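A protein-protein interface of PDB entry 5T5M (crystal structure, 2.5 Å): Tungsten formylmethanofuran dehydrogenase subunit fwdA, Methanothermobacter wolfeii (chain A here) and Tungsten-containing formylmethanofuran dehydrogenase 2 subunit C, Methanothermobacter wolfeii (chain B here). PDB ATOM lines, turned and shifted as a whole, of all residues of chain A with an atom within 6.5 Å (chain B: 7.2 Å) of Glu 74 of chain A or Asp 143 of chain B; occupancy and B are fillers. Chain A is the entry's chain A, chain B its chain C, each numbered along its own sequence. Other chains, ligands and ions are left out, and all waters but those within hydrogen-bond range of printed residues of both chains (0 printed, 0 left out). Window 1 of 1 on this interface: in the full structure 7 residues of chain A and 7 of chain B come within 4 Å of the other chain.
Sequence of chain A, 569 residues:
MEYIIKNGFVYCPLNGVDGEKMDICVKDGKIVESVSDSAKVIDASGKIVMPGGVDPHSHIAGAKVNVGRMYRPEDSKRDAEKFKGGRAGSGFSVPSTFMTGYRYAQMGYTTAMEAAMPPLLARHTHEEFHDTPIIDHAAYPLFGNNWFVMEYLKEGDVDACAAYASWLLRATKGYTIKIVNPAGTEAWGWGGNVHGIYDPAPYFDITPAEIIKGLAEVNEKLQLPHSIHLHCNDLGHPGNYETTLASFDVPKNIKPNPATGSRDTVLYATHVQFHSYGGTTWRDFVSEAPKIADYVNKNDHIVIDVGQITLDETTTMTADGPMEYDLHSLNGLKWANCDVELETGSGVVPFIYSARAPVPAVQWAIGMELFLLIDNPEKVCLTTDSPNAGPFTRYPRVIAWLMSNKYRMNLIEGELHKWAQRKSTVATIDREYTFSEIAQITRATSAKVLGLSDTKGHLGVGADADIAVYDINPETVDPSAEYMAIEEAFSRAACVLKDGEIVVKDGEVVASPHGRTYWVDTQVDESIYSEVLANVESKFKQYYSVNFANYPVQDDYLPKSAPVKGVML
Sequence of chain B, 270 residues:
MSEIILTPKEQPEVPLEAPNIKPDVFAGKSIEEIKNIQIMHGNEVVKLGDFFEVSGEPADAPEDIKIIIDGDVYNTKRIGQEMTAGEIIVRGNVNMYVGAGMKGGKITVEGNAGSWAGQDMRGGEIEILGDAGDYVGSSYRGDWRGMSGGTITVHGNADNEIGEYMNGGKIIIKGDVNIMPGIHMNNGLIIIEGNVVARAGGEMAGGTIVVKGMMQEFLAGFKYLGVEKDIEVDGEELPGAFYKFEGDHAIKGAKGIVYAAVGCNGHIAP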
ATOM      1  N   TYR A  71     -10.745  14.406 -23.445  1.00  0.00           N
ATOM      2  CA  TYR A  71     -10.047  14.345 -22.176  1.00  0.00           C
ATOM      3  C   TYR A  71      -8.711  13.612 -22.290  1.00  0.00           C
ATOM      4  O   TYR A  71      -8.063  13.372 -21.267  1.00  0.00           O
ATOM      5  CB  TYR A  71     -10.986  13.749 -21.099  1.00  0.00           C
ATOM      6  CG  TYR A  71     -10.929  12.257 -20.766  1.00  0.00           C
ATOM      7  CD1 TYR A  71     -10.749  11.291 -21.740  1.00  0.00           C
ATOM      8  CD2 TYR A  71     -11.101  11.831 -19.451  1.00  0.00           C
ATOM      9  CE1 TYR A  71     -10.720   9.950 -21.416  1.00  0.00           C
ATOM     10  CE2 TYR A  71     -11.072  10.497 -19.116  1.00  0.00           C
ATOM     11  CZ  TYR A  71     -10.879   9.557 -20.095  1.00  0.00           C
ATOM     12  OH  TYR A  71     -10.850   8.220 -19.756  1.00  0.00           O
ATOM     13  N   ARG A  72      -8.265  13.303 -23.514  1.00  0.00           N
ATOM     14  CA  ARG A  72      -6.935  12.740 -23.763  1.00  0.00           C
ATOM     15  C   ARG A  72      -6.194  13.580 -24.798  1.00  0.00           C
ATOM     16  O   ARG A  72      -5.898  13.115 -25.906  1.00  0.00           O
ATOM     17  CB  ARG A  72      -7.018  11.292 -24.240  1.00  0.00           C
ATOM     18  CG  ARG A  72      -7.668  10.342 -23.269  1.00  0.00           C
ATOM     19  CD  ARG A  72      -7.110   8.935 -23.435  1.00  0.00           C
ATOM     20  NE  ARG A  72      -5.702   8.867 -23.048  1.00  0.00           N
ATOM     21  CZ  ARG A  72      -4.926   7.800 -23.205  1.00  0.00           C
ATOM     22  NH1 ARG A  72      -5.410   6.686 -23.751  1.00  0.00           N
ATOM     23  NH2 ARG A  72      -3.656   7.845 -22.811  1.00  0.00           N
ATOM     24  N   PRO A  73      -5.854  14.822 -24.462  1.00  0.00           N
ATOM     25  CA  PRO A  73      -4.999  15.593 -25.378  1.00  0.00           C
ATOM     26  C   PRO A  73      -3.647  14.945 -25.584  1.00  0.00           C
ATOM     27  O   PRO A  73      -3.031  15.144 -26.638  1.00  0.00           O
ATOM     28  CB  PRO A  73      -4.879  16.957 -24.684  1.00  0.00           C
ATOM     29  CG  PRO A  73      -5.120  16.672 -23.246  1.00  0.00           C
ATOM     30  CD  PRO A  73      -6.097  15.534 -23.196  1.00  0.00           C
ATOM     31  N   GLU A  74      -3.179  14.161 -24.605  1.00  0.00           N
ATOM     32  CA  GLU A  74      -1.889  13.487 -24.731  1.00  0.00           C
ATOM     33  C   GLU A  74      -1.949  12.355 -25.761  1.00  0.00           C
ATOM     34  O   GLU A  74      -0.933  12.040 -26.392  1.00  0.00           O
ATOM     35  CB  GLU A  74      -1.428  12.984 -23.348  1.00  0.00           C
ATOM     36  CG  GLU A  74      -2.118  11.726 -22.811  1.00  0.00           C
ATOM     37  CD  GLU A  74      -3.547  11.958 -22.338  1.00  0.00           C
ATOM     38  OE1 GLU A  74      -4.054  13.101 -22.437  1.00  0.00           O
ATOM     39  OE2 GLU A  74      -4.168  10.978 -21.867  1.00  0.00           O
ATOM     40  N   ASP A  75      -3.121  11.744 -25.951  1.00  0.00           N
ATOM     41  CA  ASP A  75      -3.301  10.778 -27.034  1.00  0.00           C
ATOM     42  C   ASP A  75      -3.221  11.468 -28.391  1.00  0.00           C
ATOM     43  O   ASP A  75      -2.618  10.945 -29.335  1.00  0.00           O
ATOM     44  CB  ASP A  75      -4.643  10.054 -26.850  1.00  0.00           C
ATOM     45  CG  ASP A  75      -4.962   9.076 -27.972  1.00  0.00           C
ATOM     46  OD1 ASP A  75      -4.250   8.053 -28.089  1.00  0.00           O
ATOM     47  OD2 ASP A  75      -5.947   9.313 -28.719  1.00  0.00           O
ATOM     48  N   SER A  76      -3.801  12.662 -28.495  1.00  0.00           N
ATOM     49  CA  SER A  76      -3.657  13.452 -29.712  1.00  0.00           C
ATOM     50  C   SER A  76      -2.204  13.864 -29.955  1.00  0.00           C
ATOM     51  O   SER A  76      -1.731  13.852 -31.096  1.00  0.00           O
ATOM     52  CB  SER A  76      -4.562  14.680 -29.631  1.00  0.00           C
ATOM     53  OG  SER A  76      -5.920  14.321 -29.789  1.00  0.00           O
ATOM     54  N   LYS A  77      -1.474  14.238 -28.899  1.00  0.00           N
ATOM     55  CA  LYS A  77      -0.104  14.719 -29.097  1.00  0.00           C
ATOM     56  C   LYS A  77       0.825  13.596 -29.538  1.00  0.00           C
ATOM     57  O   LYS A  77       1.819  13.839 -30.229  1.00  0.00           O
ATOM     58  CB  LYS A  77       0.425  15.356 -27.816  1.00  0.00           C
ATOM     59  CG  LYS A  77       1.801  15.959 -27.983  1.00  0.00           C
ATOM     60  CD  LYS A  77       2.255  16.665 -26.739  1.00  0.00           C
ATOM     61  CE  LYS A  77       3.713  17.056 -26.828  1.00  0.00           C
ATOM     62  NZ  LYS A  77       4.373  16.841 -25.501  1.00  0.00           N
ATOM     63  N   ARG A  78       0.512  12.371 -29.139  1.00  0.00           N
ATOM     64  CA  ARG A  78       1.271  11.207 -29.565  1.00  0.00           C
ATOM     65  C   ARG A  78       1.195  10.980 -31.073  1.00  0.00           C
ATOM     66  O   ARG A  78       2.147  10.463 -31.668  1.00  0.00           O
ATOM     67  CB  ARG A  78       0.734   9.999 -28.810  1.00  0.00           C
ATOM     68  CG  ARG A  78       1.463   8.725 -29.040  1.00  0.00           C
ATOM     69  CD  ARG A  78       0.905   7.643 -28.150  1.00  0.00           C
ATOM     70  NE  ARG A  78       1.252   6.326 -28.654  1.00  0.00           N
ATOM     71  CZ  ARG A  78       0.754   5.192 -28.184  1.00  0.00           C
ATOM     72  NH1 ARG A  78      -0.125   5.215 -27.185  1.00  0.00           N
ATOM     73  NH2 ARG A  78       1.134   4.041 -28.726  1.00  0.00           N
ATOM     74  N   ASP A  79       0.070  11.357 -31.710  1.00  0.00           N
ATOM     75  CA  ASP A  79      -0.241  10.950 -33.087  1.00  0.00           C
ATOM     76  C   ASP A  79      -1.109  12.041 -33.733  1.00  0.00           C
ATOM     77  O   ASP A  79      -2.336  11.947 -33.806  1.00  0.00           O
ATOM     78  CB  ASP A  79      -0.942   9.591 -33.116  1.00  0.00           C
ATOM     79  CG  ASP A  79      -1.064   9.026 -34.515  1.00  0.00           C
ATOM     80  OD1 ASP A  79      -0.912   9.800 -35.476  1.00  0.00           O
ATOM     81  OD2 ASP A  79      -1.320   7.810 -34.654  1.00  0.00           O
ATOM     82  N   GLU A 313      -1.059   0.920 -25.291  1.00  0.00           N
ATOM     83  CA  GLU A 313      -1.758   1.902 -24.476  1.00  0.00           C
ATOM     84  C   GLU A 313      -2.946   2.394 -25.287  1.00  0.00           C
ATOM     85  O   GLU A 313      -2.767   2.965 -26.370  1.00  0.00           O
ATOM     86  CB  GLU A 313      -0.861   3.078 -24.107  1.00  0.00           C
ATOM     87  CG  GLU A 313      -1.629   4.229 -23.469  1.00  0.00           C
ATOM     88  CD  GLU A 313      -0.743   5.357 -22.972  1.00  0.00           C
ATOM     89  OE1 GLU A 313       0.466   5.128 -22.753  1.00  0.00           O
ATOM     90  OE2 GLU A 313      -1.268   6.479 -22.800  1.00  0.00           O
ATOM     91  N   LYS A 334      -7.676   8.421 -15.109  1.00  0.00           N
ATOM     92  CA  LYS A 334      -8.808   9.334 -15.210  1.00  0.00           C
ATOM     93  C   LYS A 334     -10.054   8.646 -15.762  1.00  0.00           C
ATOM     94  O   LYS A 334     -10.001   7.898 -16.742  1.00  0.00           O
ATOM     95  CB  LYS A 334      -8.448  10.527 -16.092  1.00  0.00           C
ATOM     96  CG  LYS A 334      -7.935  10.167 -17.470  1.00  0.00           C
ATOM     97  CD  LYS A 334      -7.165  11.358 -18.067  1.00  0.00           C
ATOM     98  CE  LYS A 334      -6.494  11.010 -19.379  1.00  0.00           C
ATOM     99  NZ  LYS A 334      -5.849  12.203 -19.963  1.00  0.00           N
ATOM    100  N   PRO A 350      -8.560   5.325 -19.619  1.00  0.00           N
ATOM    101  CA  PRO A 350      -7.385   4.811 -20.333  1.00  0.00           C
ATOM    102  C   PRO A 350      -6.987   3.457 -19.774  1.00  0.00           C
ATOM    103  O   PRO A 350      -7.277   3.134 -18.620  1.00  0.00           O
ATOM    104  CB  PRO A 350      -6.300   5.872 -20.070  1.00  0.00           C
ATOM    105  CG  PRO A 350      -7.022   7.075 -19.560  1.00  0.00           C
ATOM    106  CD  PRO A 350      -8.246   6.543 -18.857  1.00  0.00           C
ATOM    107  N   ASP B 120       8.526  18.088 -19.318  1.00  0.00           N
ATOM    108  CA  ASP B 120       8.798  16.710 -19.718  1.00  0.00           C
ATOM    109  C   ASP B 120      10.298  16.416 -19.776  1.00  0.00           C
ATOM    110  O   ASP B 120      10.748  15.551 -20.533  1.00  0.00           O
ATOM    111  CB  ASP B 120       8.146  16.392 -21.071  1.00  0.00           C
ATOM    112  CG  ASP B 120       6.650  16.180 -20.970  1.00  0.00           C
ATOM    113  OD1 ASP B 120       6.201  15.481 -20.036  1.00  0.00           O
ATOM    114  OD2 ASP B 120       5.930  16.709 -21.841  1.00  0.00           O
ATOM    115  N   ARG B 122      13.751  14.820 -19.291  1.00  0.00           N
ATOM    116  CA  ARG B 122      14.181  13.452 -19.047  1.00  0.00           C
ATOM    117  C   ARG B 122      15.555  13.371 -18.413  1.00  0.00           C
ATOM    118  O   ARG B 122      15.819  12.427 -17.667  1.00  0.00           O
ATOM    119  CB  ARG B 122      14.202  12.660 -20.360  1.00  0.00           C
ATOM    120  CG  ARG B 122      12.896  12.668 -21.129  1.00  0.00           C
ATOM    121  CD  ARG B 122      11.859  11.776 -20.463  1.00  0.00           C
ATOM    122  NE  ARG B 122      10.518  11.999 -21.018  1.00  0.00           N
ATOM    123  CZ  ARG B 122       9.442  12.352 -20.313  1.00  0.00           C
ATOM    124  NH1 ARG B 122       9.508  12.512 -18.994  1.00  0.00           N
ATOM    125  NH2 ARG B 122       8.279  12.538 -20.932  1.00  0.00           N
ATOM    126  N   SER B 139       4.314  18.476 -16.746  1.00  0.00           N
ATOM    127  CA  SER B 139       3.870  17.540 -17.767  1.00  0.00           C
ATOM    128  C   SER B 139       3.096  18.289 -18.847  1.00  0.00           C
ATOM    129  O   SER B 139       2.926  19.510 -18.800  1.00  0.00           O
ATOM    130  CB  SER B 139       2.994  16.456 -17.147  1.00  0.00           C
ATOM    131  OG  SER B 139       1.747  16.988 -16.733  1.00  0.00           O
ATOM    132  N   TYR B 140       2.612  17.538 -19.830  1.00  0.00           N
ATOM    133  CA  TYR B 140       1.705  18.068 -20.837  1.00  0.00           C
ATOM    134  C   TYR B 140       0.260  17.791 -20.427  1.00  0.00           C
ATOM    135  O   TYR B 140      -0.023  16.833 -19.704  1.00  0.00           O
ATOM    136  CB  TYR B 140       1.999  17.452 -22.202  1.00  0.00           C
ATOM    137  CG  TYR B 140       1.083  17.952 -23.294  1.00  0.00           C
ATOM    138  CD1 TYR B 140       1.248  19.226 -23.835  1.00  0.00           C
ATOM    139  CD2 TYR B 140       0.042  17.155 -23.774  1.00  0.00           C
ATOM    140  CE1 TYR B 140       0.401  19.694 -24.839  1.00  0.00           C
ATOM    141  CE2 TYR B 140      -0.811  17.609 -24.781  1.00  0.00           C
ATOM    142  CZ  TYR B 140      -0.627  18.881 -25.311  1.00  0.00           C
ATOM    143  OH  TYR B 140      -1.477  19.328 -26.308  1.00  0.00           O
ATOM    144  N   ARG B 141      -0.649  18.650 -20.884  1.00  0.00           N
ATOM    145  CA  ARG B 141      -2.066  18.491 -20.574  1.00  0.00           C
ATOM    146  C   ARG B 141      -2.517  17.048 -20.774  1.00  0.00           C
ATOM    147  O   ARG B 141      -2.260  16.439 -21.814  1.00  0.00           O
ATOM    148  CB  ARG B 141      -2.908  19.418 -21.459  1.00  0.00           C
ATOM    149  CG  ARG B 141      -2.541  20.883 -21.397  1.00  0.00           C
ATOM    150  CD  ARG B 141      -2.599  21.448 -19.977  1.00  0.00           C
ATOM    151  NE  ARG B 141      -2.414  22.896 -19.978  1.00  0.00           N
ATOM    152  CZ  ARG B 141      -2.399  23.663 -18.894  1.00  0.00           C
ATOM    153  NH1 ARG B 141      -2.558  23.147 -17.684  1.00  0.00           N
ATOM    154  NH2 ARG B 141      -2.222  24.962 -19.026  1.00  0.00           N
ATOM    155  N   GLY B 142      -3.208  16.510 -19.771  1.00  0.00           N
ATOM    156  CA  GLY B 142      -3.798  15.191 -19.846  1.00  0.00           C
ATOM    157  C   GLY B 142      -2.870  14.061 -19.450  1.00  0.00           C
ATOM    158  O   GLY B 142      -3.332  13.032 -18.945  1.00  0.00           O
ATOM    159  N   ASP B 143      -1.575  14.226 -19.666  1.00  0.00           N
ATOM    160  CA  ASP B 143      -0.634  13.161 -19.373  1.00  0.00           C
ATOM    161  C   ASP B 143      -0.297  13.182 -17.888  1.00  0.00           C
ATOM    162  O   ASP B 143       0.127  14.213 -17.354  1.00  0.00           O
ATOM    163  CB  ASP B 143       0.628  13.316 -20.223  1.00  0.00           C
ATOM    164  CG  ASP B 143       1.376  12.010 -20.409  1.00  0.00           C
ATOM    165  OD1 ASP B 143       1.256  11.120 -19.542  1.00  0.00           O
ATOM    166  OD2 ASP B 143       2.098  11.881 -21.419  1.00  0.00           O
ATOM    167  N   TRP B 144      -0.498  12.044 -17.229  1.00  0.00           N
ATOM    168  CA  TRP B 144      -0.218  11.881 -15.810  1.00  0.00           C
ATOM    169  C   TRP B 144       1.234  11.485 -15.559  1.00  0.00           C
ATOM    170  O   TRP B 144       1.633  11.315 -14.399  1.00  0.00           O
ATOM    171  CB  TRP B 144      -1.174  10.835 -15.202  1.00  0.00           C
ATOM    172  CG  TRP B 144      -1.078   9.458 -15.836  1.00  0.00           C
ATOM    173  CD1 TRP B 144      -0.399   8.383 -15.347  1.00  0.00           C
ATOM    174  CD2 TRP B 144      -1.680   9.023 -17.065  1.00  0.00           C
ATOM    175  NE1 TRP B 144      -0.542   7.308 -16.183  1.00  0.00           N
ATOM    176  CE2 TRP B 144      -1.319   7.672 -17.249  1.00  0.00           C
ATOM    177  CE3 TRP B 144      -2.489   9.640 -18.027  1.00  0.00           C
ATOM    178  CZ2 TRP B 144      -1.740   6.925 -18.353  1.00  0.00           C
ATOM    179  CZ3 TRP B 144      -2.904   8.892 -19.135  1.00  0.00           C
ATOM    180  CH2 TRP B 144      -2.524   7.551 -19.282  1.00  0.00           C
ATOM    181  N   ARG B 145       2.024  11.350 -16.621  1.00  0.00           N
ATOM    182  CA  ARG B 145       3.450  11.046 -16.546  1.00  0.00           C
ATOM    183  C   ARG B 145       4.212  12.309 -16.921  1.00  0.00           C
ATOM    184  O   ARG B 145       4.178  12.741 -18.075  1.00  0.00           O
ATOM    185  CB  ARG B 145       3.792   9.891 -17.481  1.00  0.00           C
ATOM    186  CG  ARG B 145       3.068   8.601 -17.134  1.00  0.00           C
ATOM    187  CD  ARG B 145       2.864   7.721 -18.344  1.00  0.00           C
ATOM    188  NE  ARG B 145       1.955   8.324 -19.313  1.00  0.00           N
ATOM    189  CZ  ARG B 145       1.322   7.651 -20.273  1.00  0.00           C
ATOM    190  NH1 ARG B 145       1.480   6.336 -20.390  1.00  0.00           N
ATOM    191  NH2 ARG B 145       0.514   8.293 -21.107  1.00  0.00           N
ATOM    192  N   GLY B 146       4.891  12.904 -15.951  1.00  0.00           N
ATOM    193  CA  GLY B 146       5.581  14.151 -16.199  1.00  0.00           C
ATOM    194  C   GLY B 146       7.085  14.017 -16.264  1.00  0.00           C
ATOM    195  O   GLY B 146       7.617  12.997 -16.716  1.00  0.00           O
ATOM    196  N   GLU B 164       4.566  20.333 -11.719  1.00  0.00           N
ATOM    197  CA  GLU B 164       3.294  19.663 -11.940  1.00  0.00           C
ATOM    198  C   GLU B 164       3.500  18.232 -12.424  1.00  0.00           C
ATOM    199  O   GLU B 164       4.193  17.989 -13.419  1.00  0.00           O
ATOM    200  CB  GLU B 164       2.483  20.461 -12.966  1.00  0.00           C
ATOM    201  CG  GLU B 164       1.098  19.931 -13.264  1.00  0.00           C
ATOM    202  CD  GLU B 164       0.815  19.853 -14.758  1.00  0.00           C
ATOM    203  OE1 GLU B 164       1.633  19.252 -15.485  1.00  0.00           O
ATOM    204  OE2 GLU B 164      -0.219  20.396 -15.214  1.00  0.00           O
ATOM    205  N   TYR B 165       2.891  17.284 -11.708  1.00  0.00           N
ATOM    206  CA  TYR B 165       2.919  15.864 -12.064  1.00  0.00           C
ATOM    207  C   TYR B 165       4.349  15.332 -12.153  1.00  0.00           C
ATOM    208  O   TYR B 165       4.615  14.360 -12.859  1.00  0.00           O
ATOM    209  CB  TYR B 165       2.163  15.602 -13.376  1.00  0.00           C
ATOM    210  CG  TYR B 165       0.670  15.385 -13.211  1.00  0.00           C
ATOM    211  CD1 TYR B 165       0.177  14.202 -12.681  1.00  0.00           C
ATOM    212  CD2 TYR B 165      -0.247  16.351 -13.605  1.00  0.00           C
ATOM    213  CE1 TYR B 165      -1.174  13.994 -12.529  1.00  0.00           C
ATOM    214  CE2 TYR B 165      -1.620  16.149 -13.456  1.00  0.00           C
ATOM    215  CZ  TYR B 165      -2.069  14.972 -12.921  1.00  0.00           C
ATOM    216  OH  TYR B 165      -3.415  14.759 -12.769  1.00  0.00           O
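Printed residues of chain A that touch a printed residue of chain B: Arg 72, Pro 73, Glu 74, Lys 77, Glu 313 and Lys 334. Hydrophobic or aromatic side chains of chain A that line the printed part of chain B: Pro 73. Of the 12 printed residues of chain B, 7 touch a printed residue of chain A. Hydrophobic or aromatic side chains of chain B within 4 Å of the printed part of chain A: Tyr 140 and Trp 144. Among the printed residues, Asp or Glu carboxylates within 4 Å of a Lys or Arg side-chain nitrogen of the other chain: Lys 77 of chain A with Asp 120 of chain B (3.98 Å) and Glu 313 of chain A with Arg 145 of chain B (2.8 Å).
O of Tyr 71 of chain A lies within hydrogen-bond range of NZ of Lys 334 of chain A, 2.8 Å away. The side-chain carboxylate of Glu 74 of chain A lies within salt-bridge range of the side-chain amino group of Lys 334 of chain A. The guanidinium group (NH2) of Arg 122 of chain B lies within salt-bridge range of the side-chain carboxylate (OD1) of Asp 120 of chain B (3.7 Å). The guanidinium group of Arg 72 of chain A is in salt-bridge range of the side-chain carboxylate of Glu 74 of chain A (2.9 Å). The guanidinium group (NH2) of Arg 72 of chain A lies within salt-bridge range of the side-chain carboxylate (OE2) of Glu 313 of chain A, 2.8 Å away. The side-chain carboxylate (OD1) of Asp 143 of chain B lies within salt-bridge range of the guanidinium group (NE) of Arg 145 of chain B.
Tyr 71 of chain A touches none of the printed residues of chain B. Printed residues of chain B within 4 Å of Arg 72 of chain A: Trp 144. Of the printed residues of chain B, Pro 73 of chain A touches Tyr 140 (3.8 Å), Arg 141 (3.2 Å) and Gly 142 (3.9 Å). Glu 74 of chain A touches four residues of chain B. Of the printed residues of chain B, Glu 313 of chain A touches Trp 144 (3.9 Å) and Arg 145 (2.8 Å). Of the printed residues of chain B, Lys 334 of chain A touches Gly 142 (2.8 Å). Of the printed residues of chain A, Tyr 140 of chain B touches Pro 73 (3.8 Å) and Lys 77 (3.7 Å). Of chain A, only Glu 74 (3.8 Å) comes within 4 Å of Asp 143 of chain B. The nearest residue of chain B that does not touch Glu 74 of chain A is Tyr 140 of chain B (4.2 Å). The nearest residue of chain A that does not touch Asp 143 of chain B is Lys 334 of chain A (4.7 Å).
Among the printed residues, pairs that only touch across the chains: Pro 73 of chain A with Arg 141 of chain B (3.2 Å), Glu 74 of chain A with Gly 142 of chain B (3.3 Å), Glu 74 of chain A with Trp 144 of chain B (3.7 Å), Arg 72 of chain A with Trp 144 of chain B (3.7 Å), Glu 74 of chain A with Arg 141 of chain B (3.7 Å), Lys 77 of chain A with Tyr 140 of chain B (3.7 Å), Glu 74 of chain A with Asp 143 of chain B (3.8 Å), Pro 73 of chain A with Tyr 140 of chain B (3.8 Å), Glu 313 of chain A with Trp 144 of chain B (3.9 Å) and Pro 73 of chain A with Gly 142 of chain B (3.9 Å).
O of Gly 142 of chain B lies within hydrogen-bond range of NZ of Lys 334 of chain A (2.8 Å). NZ of Lys 77 of chain A is in salt-bridge range of OD2 of Asp 120 of chain B. OE1 of Glu 313 of chain A lies within salt-bridge range of NH1 of Arg 145 of chain B (2.8 Å).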
